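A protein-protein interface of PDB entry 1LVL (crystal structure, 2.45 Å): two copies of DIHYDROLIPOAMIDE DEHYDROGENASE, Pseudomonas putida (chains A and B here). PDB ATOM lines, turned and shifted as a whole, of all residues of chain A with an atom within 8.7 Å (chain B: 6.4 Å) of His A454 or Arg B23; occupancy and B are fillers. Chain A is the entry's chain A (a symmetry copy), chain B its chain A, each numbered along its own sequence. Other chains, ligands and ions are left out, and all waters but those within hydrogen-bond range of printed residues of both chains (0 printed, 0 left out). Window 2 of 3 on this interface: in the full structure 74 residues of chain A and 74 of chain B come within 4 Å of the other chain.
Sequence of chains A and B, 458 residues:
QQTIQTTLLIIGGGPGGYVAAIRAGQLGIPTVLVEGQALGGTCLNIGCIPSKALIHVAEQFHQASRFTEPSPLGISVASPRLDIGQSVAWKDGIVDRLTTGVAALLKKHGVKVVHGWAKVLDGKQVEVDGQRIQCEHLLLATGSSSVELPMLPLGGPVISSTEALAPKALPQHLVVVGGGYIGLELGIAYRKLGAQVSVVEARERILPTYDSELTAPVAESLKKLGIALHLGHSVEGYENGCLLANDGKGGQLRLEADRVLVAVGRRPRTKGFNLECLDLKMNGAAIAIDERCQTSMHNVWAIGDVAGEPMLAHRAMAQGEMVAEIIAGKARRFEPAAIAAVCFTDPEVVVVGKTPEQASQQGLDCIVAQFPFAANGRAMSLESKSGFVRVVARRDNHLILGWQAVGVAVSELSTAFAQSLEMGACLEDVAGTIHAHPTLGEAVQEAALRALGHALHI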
ATOM      1  N   GLU A 428       3.595   7.188   5.151  1.00  0.00           N
ATOM      2  CA  GLU A 428       4.277   6.594   4.000  1.00  0.00           C
ATOM      3  C   GLU A 428       5.651   7.160   3.625  1.00  0.00           C
ATOM      4  O   GLU A 428       6.604   6.451   3.315  1.00  0.00           O
ATOM      5  CB  GLU A 428       3.444   6.716   2.733  1.00  0.00           C
ATOM      6  CG  GLU A 428       2.184   5.911   2.538  1.00  0.00           C
ATOM      7  CD  GLU A 428       0.880   6.600   2.918  1.00  0.00           C
ATOM      8  OE1 GLU A 428       0.268   7.264   2.062  1.00  0.00           O
ATOM      9  OE2 GLU A 428       0.474   6.434   4.067  1.00  0.00           O
ATOM     10  N   ALA A 431       8.108   6.245   6.499  1.00  0.00           N
ATOM     11  CA  ALA A 431       8.307   4.803   6.459  1.00  0.00           C
ATOM     12  C   ALA A 431       9.128   4.425   5.225  1.00  0.00           C
ATOM     13  O   ALA A 431      10.028   3.582   5.244  1.00  0.00           O
ATOM     14  CB  ALA A 431       6.955   4.136   6.384  1.00  0.00           C
ATOM     15  N   GLY A 432       8.849   5.078   4.108  1.00  0.00           N
ATOM     16  CA  GLY A 432       9.562   4.798   2.883  1.00  0.00           C
ATOM     17  C   GLY A 432      10.854   5.591   2.748  1.00  0.00           C
ATOM     18  O   GLY A 432      11.246   5.944   1.638  1.00  0.00           O
ATOM     19  N   GLN A 445      11.092   5.369  11.793  1.00  0.00           N
ATOM     20  CA  GLN A 445      10.626   4.700  10.579  1.00  0.00           C
ATOM     21  C   GLN A 445       9.718   3.514  10.936  1.00  0.00           C
ATOM     22  O   GLN A 445       8.645   3.330  10.379  1.00  0.00           O
ATOM     23  CB  GLN A 445      11.801   4.192   9.805  1.00  0.00           C
ATOM     24  CG  GLN A 445      11.379   3.751   8.403  1.00  0.00           C
ATOM     25  CD  GLN A 445      12.418   2.855   7.734  1.00  0.00           C
ATOM     26  OE1 GLN A 445      13.474   2.493   8.267  1.00  0.00           O
ATOM     27  NE2 GLN A 445      12.164   2.417   6.526  1.00  0.00           N
ATOM     28  N   GLU A 446      10.113   2.687  11.891  1.00  0.00           N
ATOM     29  CA  GLU A 446       9.310   1.585  12.373  1.00  0.00           C
ATOM     30  C   GLU A 446       7.990   2.022  13.005  1.00  0.00           C
ATOM     31  O   GLU A 446       6.975   1.417  12.636  1.00  0.00           O
ATOM     32  CB  GLU A 446      10.099   0.799  13.373  1.00  0.00           C
ATOM     33  CG  GLU A 446      11.292  -0.053  12.880  1.00  0.00           C
ATOM     34  CD  GLU A 446      10.883  -1.354  12.217  1.00  0.00           C
ATOM     35  OE1 GLU A 446      10.530  -1.369  11.029  1.00  0.00           O
ATOM     36  OE2 GLU A 446      10.904  -2.353  12.922  1.00  0.00           O
ATOM     37  N   ALA A 447       7.906   3.043  13.889  1.00  0.00           N
ATOM     38  CA  ALA A 447       6.630   3.538  14.421  1.00  0.00           C
ATOM     39  C   ALA A 447       5.726   3.939  13.267  1.00  0.00           C
ATOM     40  O   ALA A 447       4.510   3.746  13.338  1.00  0.00           O
ATOM     41  CB  ALA A 447       6.846   4.734  15.286  1.00  0.00           C
ATOM     42  N   ALA A 448       6.244   4.415  12.124  1.00  0.00           N
ATOM     43  CA  ALA A 448       5.389   4.681  10.963  1.00  0.00           C
ATOM     44  C   ALA A 448       5.047   3.410  10.145  1.00  0.00           C
ATOM     45  O   ALA A 448       4.103   3.320   9.337  1.00  0.00           O
ATOM     46  CB  ALA A 448       6.088   5.633  10.036  1.00  0.00           C
ATOM     47  N   LEU A 449       5.818   2.348  10.322  1.00  0.00           N
ATOM     48  CA  LEU A 449       5.608   1.178   9.498  1.00  0.00           C
ATOM     49  C   LEU A 449       4.483   0.423  10.177  1.00  0.00           C
ATOM     50  O   LEU A 449       3.561  -0.126   9.552  1.00  0.00           O
ATOM     51  CB  LEU A 449       6.911   0.406   9.458  1.00  0.00           C
ATOM     52  CG  LEU A 449       7.562  -0.009   8.140  1.00  0.00           C
ATOM     53  CD1 LEU A 449       7.010   0.603   6.859  1.00  0.00           C
ATOM     54  CD2 LEU A 449       8.977   0.377   8.361  1.00  0.00           C
ATOM     55  N   ARG A 450       4.519   0.480  11.506  1.00  0.00           N
ATOM     56  CA  ARG A 450       3.541  -0.178  12.339  1.00  0.00           C
ATOM     57  C   ARG A 450       2.165   0.407  12.141  1.00  0.00           C
ATOM     58  O   ARG A 450       1.235  -0.373  11.989  1.00  0.00           O
ATOM     59  CB  ARG A 450       4.012  -0.039  13.742  1.00  0.00           C
ATOM     60  CG  ARG A 450       3.259  -0.959  14.602  1.00  0.00           C
ATOM     61  CD  ARG A 450       3.898  -1.026  15.974  1.00  0.00           C
ATOM     62  NE  ARG A 450       3.544  -2.345  16.477  1.00  0.00           N
ATOM     63  CZ  ARG A 450       3.607  -2.697  17.753  1.00  0.00           C
ATOM     64  NH1 ARG A 450       4.021  -1.853  18.707  1.00  0.00           N
ATOM     65  NH2 ARG A 450       3.245  -3.942  18.043  1.00  0.00           N
ATOM     66  N   ALA A 451       2.009   1.738  12.047  1.00  0.00           N
ATOM     67  CA  ALA A 451       0.717   2.387  11.820  1.00  0.00           C
ATOM     68  C   ALA A 451       0.115   1.962  10.504  1.00  0.00           C
ATOM     69  O   ALA A 451      -1.100   1.870  10.312  1.00  0.00           O
ATOM     70  CB  ALA A 451       0.849   3.902  11.783  1.00  0.00           C
ATOM     71  N   LEU A 452       1.013   1.700   9.576  1.00  0.00           N
ATOM     72  CA  LEU A 452       0.587   1.209   8.284  1.00  0.00           C
ATOM     73  C   LEU A 452       0.277  -0.299   8.280  1.00  0.00           C
ATOM     74  O   LEU A 452      -0.248  -0.866   7.311  1.00  0.00           O
ATOM     75  CB  LEU A 452       1.687   1.561   7.288  1.00  0.00           C
ATOM     76  CG  LEU A 452       1.835   3.013   6.895  1.00  0.00           C
ATOM     77  CD1 LEU A 452       3.145   3.099   6.146  1.00  0.00           C
ATOM     78  CD2 LEU A 452       0.679   3.510   6.015  1.00  0.00           C
ATOM     79  N   GLY A 453       0.603  -1.011   9.341  1.00  0.00           N
ATOM     80  CA  GLY A 453       0.289  -2.418   9.384  1.00  0.00           C
ATOM     81  C   GLY A 453       1.471  -3.325   9.115  1.00  0.00           C
ATOM     82  O   GLY A 453       1.276  -4.541   9.219  1.00  0.00           O
ATOM     83  N   HIS A 454       2.690  -2.819   8.799  1.00  0.00           N
ATOM     84  CA  HIS A 454       3.836  -3.695   8.548  1.00  0.00           C
ATOM     85  C   HIS A 454       5.268  -3.422   9.005  1.00  0.00           C
ATOM     86  O   HIS A 454       6.228  -3.259   8.238  1.00  0.00           O
ATOM     87  CB  HIS A 454       3.891  -3.987   7.071  1.00  0.00           C
ATOM     88  CG  HIS A 454       3.921  -2.843   6.120  1.00  0.00           C
ATOM     89  ND1 HIS A 454       5.070  -2.461   5.600  1.00  0.00           N
ATOM     90  CD2 HIS A 454       2.815  -2.339   5.500  1.00  0.00           C
ATOM     91  CE1 HIS A 454       4.681  -1.693   4.596  1.00  0.00           C
ATOM     92  NE2 HIS A 454       3.352  -1.620   4.537  1.00  0.00           N
ATOM     93  N   ALA A 455       5.392  -3.499  10.336  1.00  0.00           N
ATOM     94  CA  ALA A 455       6.662  -3.311  10.989  1.00  0.00           C
ATOM     95  C   ALA A 455       7.481  -4.600  10.980  1.00  0.00           C
ATOM     96  O   ALA A 455       6.979  -5.726  10.972  1.00  0.00           O
ATOM     97  CB  ALA A 455       6.474  -2.872  12.439  1.00  0.00           C
ATOM     98  N   LEU A 456       8.791  -4.383  11.037  1.00  0.00           N
ATOM     99  CA  LEU A 456       9.744  -5.439  10.861  1.00  0.00           C
ATOM    100  C   LEU A 456      10.457  -5.892  12.080  1.00  0.00           C
ATOM    101  O   LEU A 456      10.902  -7.042  12.053  1.00  0.00           O
ATOM    102  CB  LEU A 456      10.753  -5.002   9.851  1.00  0.00           C
ATOM    103  CG  LEU A 456      10.115  -4.587   8.527  1.00  0.00           C
ATOM    104  CD1 LEU A 456      10.975  -3.473   7.967  1.00  0.00           C
ATOM    105  CD2 LEU A 456       9.916  -5.803   7.577  1.00  0.00           C
ATOM    106  N   HIS A 457      10.608  -5.083  13.134  1.00  0.00           N
ATOM    107  CA  HIS A 457      11.394  -5.535  14.286  1.00  0.00           C
ATOM    108  C   HIS A 457      10.646  -5.600  15.602  1.00  0.00           C
ATOM    109  O   HIS A 457      11.213  -5.802  16.696  1.00  0.00           O
ATOM    110  CB  HIS A 457      12.589  -4.652  14.461  1.00  0.00           C
ATOM    111  CG  HIS A 457      13.543  -4.755  13.277  1.00  0.00           C
ATOM    112  ND1 HIS A 457      13.244  -4.194  12.101  1.00  0.00           N
ATOM    113  CD2 HIS A 457      14.678  -5.519  13.260  1.00  0.00           C
ATOM    114  CE1 HIS A 457      14.209  -4.620  11.304  1.00  0.00           C
ATOM    115  NE2 HIS A 457      15.039  -5.395  12.000  1.00  0.00           N
ATOM    116  N   ILE A 458       9.327  -5.470  15.423  1.00  0.00           N
ATOM    117  CA  ILE A 458       8.352  -5.626  16.494  1.00  0.00           C
ATOM    118  C   ILE A 458       7.238  -6.284  15.726  1.00  0.00           C
ATOM    119  O   ILE A 458       6.606  -7.123  16.352  1.00  0.00           O
ATOM    120  CB  ILE A 458       7.848  -4.258  17.115  1.00  0.00           C
ATOM    121  CG1 ILE A 458       7.264  -4.544  18.436  1.00  0.00           C
ATOM    122  CG2 ILE A 458       6.766  -3.556  16.308  1.00  0.00           C
ATOM    123  CD1 ILE A 458       8.315  -5.096  19.438  1.00  0.00           C
ATOM    124  OXT ILE A 458       7.024  -5.970  14.542  1.00  0.00           O
ATOM    125  N   TYR B  18      16.827 -11.605   6.496  1.00  0.00           N
ATOM    126  CA  TYR B  18      15.732 -11.744   7.404  1.00  0.00           C
ATOM    127  C   TYR B  18      14.652 -10.717   7.168  1.00  0.00           C
ATOM    128  O   TYR B  18      13.512 -11.052   7.433  1.00  0.00           O
ATOM    129  CB  TYR B  18      16.241 -11.730   8.824  1.00  0.00           C
ATOM    130  CG  TYR B  18      16.803 -10.490   9.492  1.00  0.00           C
ATOM    131  CD1 TYR B  18      16.110  -9.301   9.536  1.00  0.00           C
ATOM    132  CD2 TYR B  18      17.986 -10.600  10.188  1.00  0.00           C
ATOM    133  CE1 TYR B  18      16.566  -8.232  10.275  1.00  0.00           C
ATOM    134  CE2 TYR B  18      18.452  -9.533  10.931  1.00  0.00           C
ATOM    135  CZ  TYR B  18      17.737  -8.356  10.972  1.00  0.00           C
ATOM    136  OH  TYR B  18      18.195  -7.279  11.710  1.00  0.00           O
ATOM    137  N   VAL B  19      14.863  -9.543   6.599  1.00  0.00           N
ATOM    138  CA  VAL B  19      13.760  -8.631   6.296  1.00  0.00           C
ATOM    139  C   VAL B  19      13.127  -9.016   4.968  1.00  0.00           C
ATOM    140  O   VAL B  19      11.973  -8.654   4.717  1.00  0.00           O
ATOM    141  CB  VAL B  19      14.337  -7.150   6.308  1.00  0.00           C
ATOM    142  CG1 VAL B  19      13.373  -6.106   5.766  1.00  0.00           C
ATOM    143  CG2 VAL B  19      14.665  -6.803   7.753  1.00  0.00           C
ATOM    144  N   ALA B  20      13.792  -9.698   4.029  1.00  0.00           N
ATOM    145  CA  ALA B  20      13.096 -10.160   2.832  1.00  0.00           C
ATOM    146  C   ALA B  20      12.163 -11.256   3.340  1.00  0.00           C
ATOM    147  O   ALA B  20      10.988 -11.294   2.999  1.00  0.00           O
ATOM    148  CB  ALA B  20      14.049 -10.770   1.835  1.00  0.00           C
ATOM    149  N   ALA B  21      12.644 -12.127   4.220  1.00  0.00           N
ATOM    150  CA  ALA B  21      11.861 -13.189   4.844  1.00  0.00           C
ATOM    151  C   ALA B  21      10.635 -12.617   5.558  1.00  0.00           C
ATOM    152  O   ALA B  21       9.541 -12.806   5.030  1.00  0.00           O
ATOM    153  CB  ALA B  21      12.720 -13.952   5.890  1.00  0.00           C
ATOM    154  N   ILE B  22      10.812 -11.892   6.699  1.00  0.00           N
ATOM    155  CA  ILE B  22       9.774 -11.278   7.526  1.00  0.00           C
ATOM    156  C   ILE B  22       8.797 -10.629   6.592  1.00  0.00           C
ATOM    157  O   ILE B  22       7.659 -11.071   6.681  1.00  0.00           O
ATOM    158  CB  ILE B  22      10.375 -10.233   8.467  1.00  0.00           C
ATOM    159  CG1 ILE B  22      11.262 -10.902   9.498  1.00  0.00           C
ATOM    160  CG2 ILE B  22       9.273  -9.497   9.200  1.00  0.00           C
ATOM    161  CD1 ILE B  22      12.032  -9.837  10.385  1.00  0.00           C
ATOM    162  N   ARG B  23       9.070  -9.704   5.659  1.00  0.00           N
ATOM    163  CA  ARG B  23       8.010  -9.187   4.799  1.00  0.00           C
ATOM    164  C   ARG B  23       7.416 -10.218   3.875  1.00  0.00           C
ATOM    165  O   ARG B  23       6.232 -10.074   3.554  1.00  0.00           O
ATOM    166  CB  ARG B  23       8.453  -8.060   3.889  1.00  0.00           C
ATOM    167  CG  ARG B  23       8.063  -6.665   4.404  1.00  0.00           C
ATOM    168  CD  ARG B  23       6.918  -6.014   3.591  1.00  0.00           C
ATOM    169  NE  ARG B  23       5.605  -6.137   4.239  1.00  0.00           N
ATOM    170  CZ  ARG B  23       4.476  -5.621   3.723  1.00  0.00           C
ATOM    171  NH1 ARG B  23       4.407  -4.929   2.582  1.00  0.00           N
ATOM    172  NH2 ARG B  23       3.349  -5.814   4.390  1.00  0.00           N
ATOM    173  N   ALA B  24       8.136 -11.245   3.393  1.00  0.00           N
ATOM    174  CA  ALA B  24       7.510 -12.263   2.552  1.00  0.00           C
ATOM    175  C   ALA B  24       6.647 -13.160   3.469  1.00  0.00           C
ATOM    176  O   ALA B  24       5.494 -13.444   3.107  1.00  0.00           O
ATOM    177  CB  ALA B  24       8.581 -13.061   1.848  1.00  0.00           C
ATOM    178  N   GLY B  25       7.054 -13.623   4.656  1.00  0.00           N
ATOM    179  CA  GLY B  25       6.156 -14.276   5.598  1.00  0.00           C
ATOM    180  C   GLY B  25       4.897 -13.404   5.806  1.00  0.00           C
ATOM    181  O   GLY B  25       3.761 -13.847   5.584  1.00  0.00           O
ATOM    182  N   GLN B  26       5.084 -12.118   6.101  1.00  0.00           N
ATOM    183  CA  GLN B  26       4.006 -11.154   6.273  1.00  0.00           C
ATOM    184  C   GLN B  26       3.069 -11.085   5.089  1.00  0.00           C
ATOM    185  O   GLN B  26       1.844 -11.041   5.258  1.00  0.00           O
ATOM    186  CB  GLN B  26       4.520  -9.730   6.468  1.00  0.00           C
ATOM    187  CG  GLN B  26       5.024  -9.355   7.861  1.00  0.00           C
ATOM    188  CD  GLN B  26       5.572  -7.931   8.032  1.00  0.00           C
ATOM    189  OE1 GLN B  26       5.476  -7.069   7.166  1.00  0.00           O
ATOM    190  NE2 GLN B  26       6.191  -7.687   9.176  1.00  0.00           N
ATOM    191  N   LEU B  27       3.631 -11.035   3.887  1.00  0.00           N
ATOM    192  CA  LEU B  27       2.800 -10.948   2.702  1.00  0.00           C
ATOM    193  C   LEU B  27       2.241 -12.327   2.355  1.00  0.00           C
ATOM    194  O   LEU B  27       1.484 -12.457   1.379  1.00  0.00           O
ATOM    195  CB  LEU B  27       3.614 -10.420   1.507  1.00  0.00           C
ATOM    196  CG  LEU B  27       3.991  -8.955   1.430  1.00  0.00           C
ATOM    197  CD1 LEU B  27       5.032  -8.648   0.334  1.00  0.00           C
ATOM    198  CD2 LEU B  27       2.657  -8.232   1.265  1.00  0.00           C
ATOM    199  N   GLY B  28       2.678 -13.381   3.084  1.00  0.00           N
ATOM    200  CA  GLY B  28       2.217 -14.751   2.910  1.00  0.00           C
ATOM    201  C   GLY B  28       2.807 -15.505   1.721  1.00  0.00           C
ATOM    202  O   GLY B  28       2.108 -16.291   1.068  1.00  0.00           O
ATOM    203  N   ILE B  29       4.075 -15.302   1.378  1.00  0.00           N
ATOM    204  CA  ILE B  29       4.703 -16.091   0.335  1.00  0.00           C
ATOM    205  C   ILE B  29       5.391 -17.182   1.138  1.00  0.00           C
ATOM    206  O   ILE B  29       5.977 -16.847   2.180  1.00  0.00           O
ATOM    207  CB  ILE B  29       5.715 -15.256  -0.455  1.00  0.00           C
ATOM    208  CG1 ILE B  29       4.988 -14.269  -1.365  1.00  0.00           C
ATOM    209  CG2 ILE B  29       6.570 -16.162  -1.289  1.00  0.00           C
ATOM    210  CD1 ILE B  29       5.880 -13.124  -1.884  1.00  0.00           C
ATOM    211  N   HIS B 109       6.123 -14.990  11.929  1.00  0.00           N
ATOM    212  CA  HIS B 109       5.584 -14.938  10.574  1.00  0.00           C
ATOM    213  C   HIS B 109       5.694 -16.232   9.773  1.00  0.00           C
ATOM    214  O   HIS B 109       5.346 -16.290   8.583  1.00  0.00           O
ATOM    215  CB  HIS B 109       6.260 -13.812   9.807  1.00  0.00           C
ATOM    216  CG  HIS B 109       5.976 -12.453  10.419  1.00  0.00           C
ATOM    217  ND1 HIS B 109       4.861 -11.802  10.154  1.00  0.00           N
ATOM    218  CD2 HIS B 109       6.758 -11.840  11.347  1.00  0.00           C
ATOM    219  CE1 HIS B 109       4.940 -10.756  10.945  1.00  0.00           C
ATOM    220  NE2 HIS B 109       6.060 -10.785  11.642  1.00  0.00           N
ATOM    221  N   GLY B 320      15.819  -6.046   0.618  1.00  0.00           N
ATOM    222  CA  GLY B 320      15.063  -7.195   1.075  1.00  0.00           C
ATOM    223  C   GLY B 320      13.551  -6.921   1.031  1.00  0.00           C
ATOM    224  O   GLY B 320      12.844  -7.509   0.196  1.00  0.00           O
ATOM    225  N   GLU B 321      13.045  -5.987   1.858  1.00  0.00           N
ATOM    226  CA  GLU B 321      11.636  -5.688   1.864  1.00  0.00           C
ATOM    227  C   GLU B 321      11.139  -5.383   0.468  1.00  0.00           C
ATOM    228  O   GLU B 321      10.048  -5.866   0.184  1.00  0.00           O
ATOM    229  CB  GLU B 321      11.382  -4.532   2.820  1.00  0.00           C
ATOM    230  CG  GLU B 321      10.640  -3.269   2.288  1.00  0.00           C
ATOM    231  CD  GLU B 321       9.826  -2.482   3.321  1.00  0.00           C
ATOM    232  OE1 GLU B 321      10.394  -1.835   4.206  1.00  0.00           O
ATOM    233  OE2 GLU B 321       8.601  -2.511   3.240  1.00  0.00           O
ATOM    234  N   ALA B 324      10.683  -8.661  -1.702  1.00  0.00           N
ATOM    235  CA  ALA B 324       9.567  -9.401  -1.146  1.00  0.00           C
ATOM    236  C   ALA B 324       8.276  -8.887  -1.735  1.00  0.00           C
ATOM    237  O   ALA B 324       7.531  -9.642  -2.362  1.00  0.00           O
ATOM    238  CB  ALA B 324       9.605  -9.261   0.380  1.00  0.00           C
ATOM    239  N   GLU B 325       8.069  -7.585  -1.716  1.00  0.00           N
ATOM    240  CA  GLU B 325       6.867  -7.019  -2.298  1.00  0.00           C
ATOM    241  C   GLU B 325       6.772  -7.211  -3.801  1.00  0.00           C
ATOM    242  O   GLU B 325       5.647  -7.357  -4.277  1.00  0.00           O
ATOM    243  CB  GLU B 325       6.786  -5.528  -2.007  1.00  0.00           C
ATOM    244  CG  GLU B 325       6.996  -5.115  -0.536  1.00  0.00           C
ATOM    245  CD  GLU B 325       6.908  -3.600  -0.250  1.00  0.00           C
ATOM    246  OE1 GLU B 325       6.488  -2.830  -1.123  1.00  0.00           O
ATOM    247  OE2 GLU B 325       7.267  -3.185   0.858  1.00  0.00           O
ATOM    248  N   LYS B 330       3.426  -6.421  -5.993  1.00  0.00           N
ATOM    249  CA  LYS B 330       3.519  -4.962  -6.012  1.00  0.00           C
ATOM    250  C   LYS B 330       4.609  -4.479  -6.955  1.00  0.00           C
ATOM    251  O   LYS B 330       5.676  -5.099  -7.064  1.00  0.00           O
ATOM    252  CB  LYS B 330       3.784  -4.465  -4.603  1.00  0.00           C
ATOM    253  CG  LYS B 330       2.517  -4.581  -3.781  1.00  0.00           C
ATOM    254  CD  LYS B 330       2.877  -4.635  -2.305  1.00  0.00           C
ATOM    255  CE  LYS B 330       1.684  -5.032  -1.448  1.00  0.00           C
ATOM    256  NZ  LYS B 330       1.167  -6.331  -1.842  1.00  0.00           N
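The side-chain amide nitrogen (NE2) of Gln B26 is in hydrogen-bond range of the backbone carbonyl oxygen (O) of Ala A455 (2.8 Å).
The side-chain carboxylate of Glu A446 sits at hydrogen-bond distance from the backbone NH of Leu A456 (3.5 Å).
OE2 of Glu A446 is in hydrogen-bond range of N of His A457.
The backbone carbonyl oxygen of Leu A449 lies within hydrogen-bond range of the backbone NH of His A454 (2.9 Å).
The guanidinium group (NE) of Arg B23 sits at hydrogen-bond distance from the side-chain amide oxygen (OE1) of Gln B26.
The side-chain carboxylate (OE2) of Glu B325 lies within salt-bridge range of the guanidinium group (NH1) of Arg B23, 3.8 Å away.
Among the printed residues, merely in contact across the chains: His A454 with Arg B23, His A454 with Gln B26, Leu A456 with Val B19, Leu A456 with Ile B22, Leu A456 with Arg B23 and His A457 with Tyr B18.
His A454 touches just these residues of chain B: Arg B23 (3.3 Å) and Gln B26 (3.5 Å).
Arg B23 touches two residues of chain A.
No residue of chain A comes within 4 Å of Ala B24.
Printed residues of chain A within 4 Å of Val B19: Leu A456.
Printed residues of chain B within 4 Å of Ala A455: Gln B26 (2.8 Å).
Printed residues of chain B within 4 Å of Leu A456: Val B19 (3.9 Å), Ile B22 (3.4 Å) and Arg B23 (3.8 Å).
Glu B321 touches none of the printed residues of chain A.
Gln A445 touches none of the printed residues of chain B.
The nearest residue of chain B that does not touch His A454 is Glu B321 (4.2 Å).
The nearest residue of chain A that does not touch Arg B23 is Gly A453 (5.4 Å).
Printed residues of chain A that touch a printed residue of chain B: His A454, Ala A455, Leu A456 and His A457.
Along chain A the printed residues that touch a printed residue of chain B span positions 454 to 457.
Along chain B the printed residues that touch a printed residue of chain A span positions 18 to 26.
Among the printed residues, 7 pairs touch across the chains.
Among the printed residues, no Asp or Glu carboxylate lies within 4 Å of a Lys or Arg side-chain nitrogen of the other chain.
No position is printed for both chains.
Of the 7 pairs that touch across the chains among the printed residues, none has its exchanged pair printed and touching as well.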
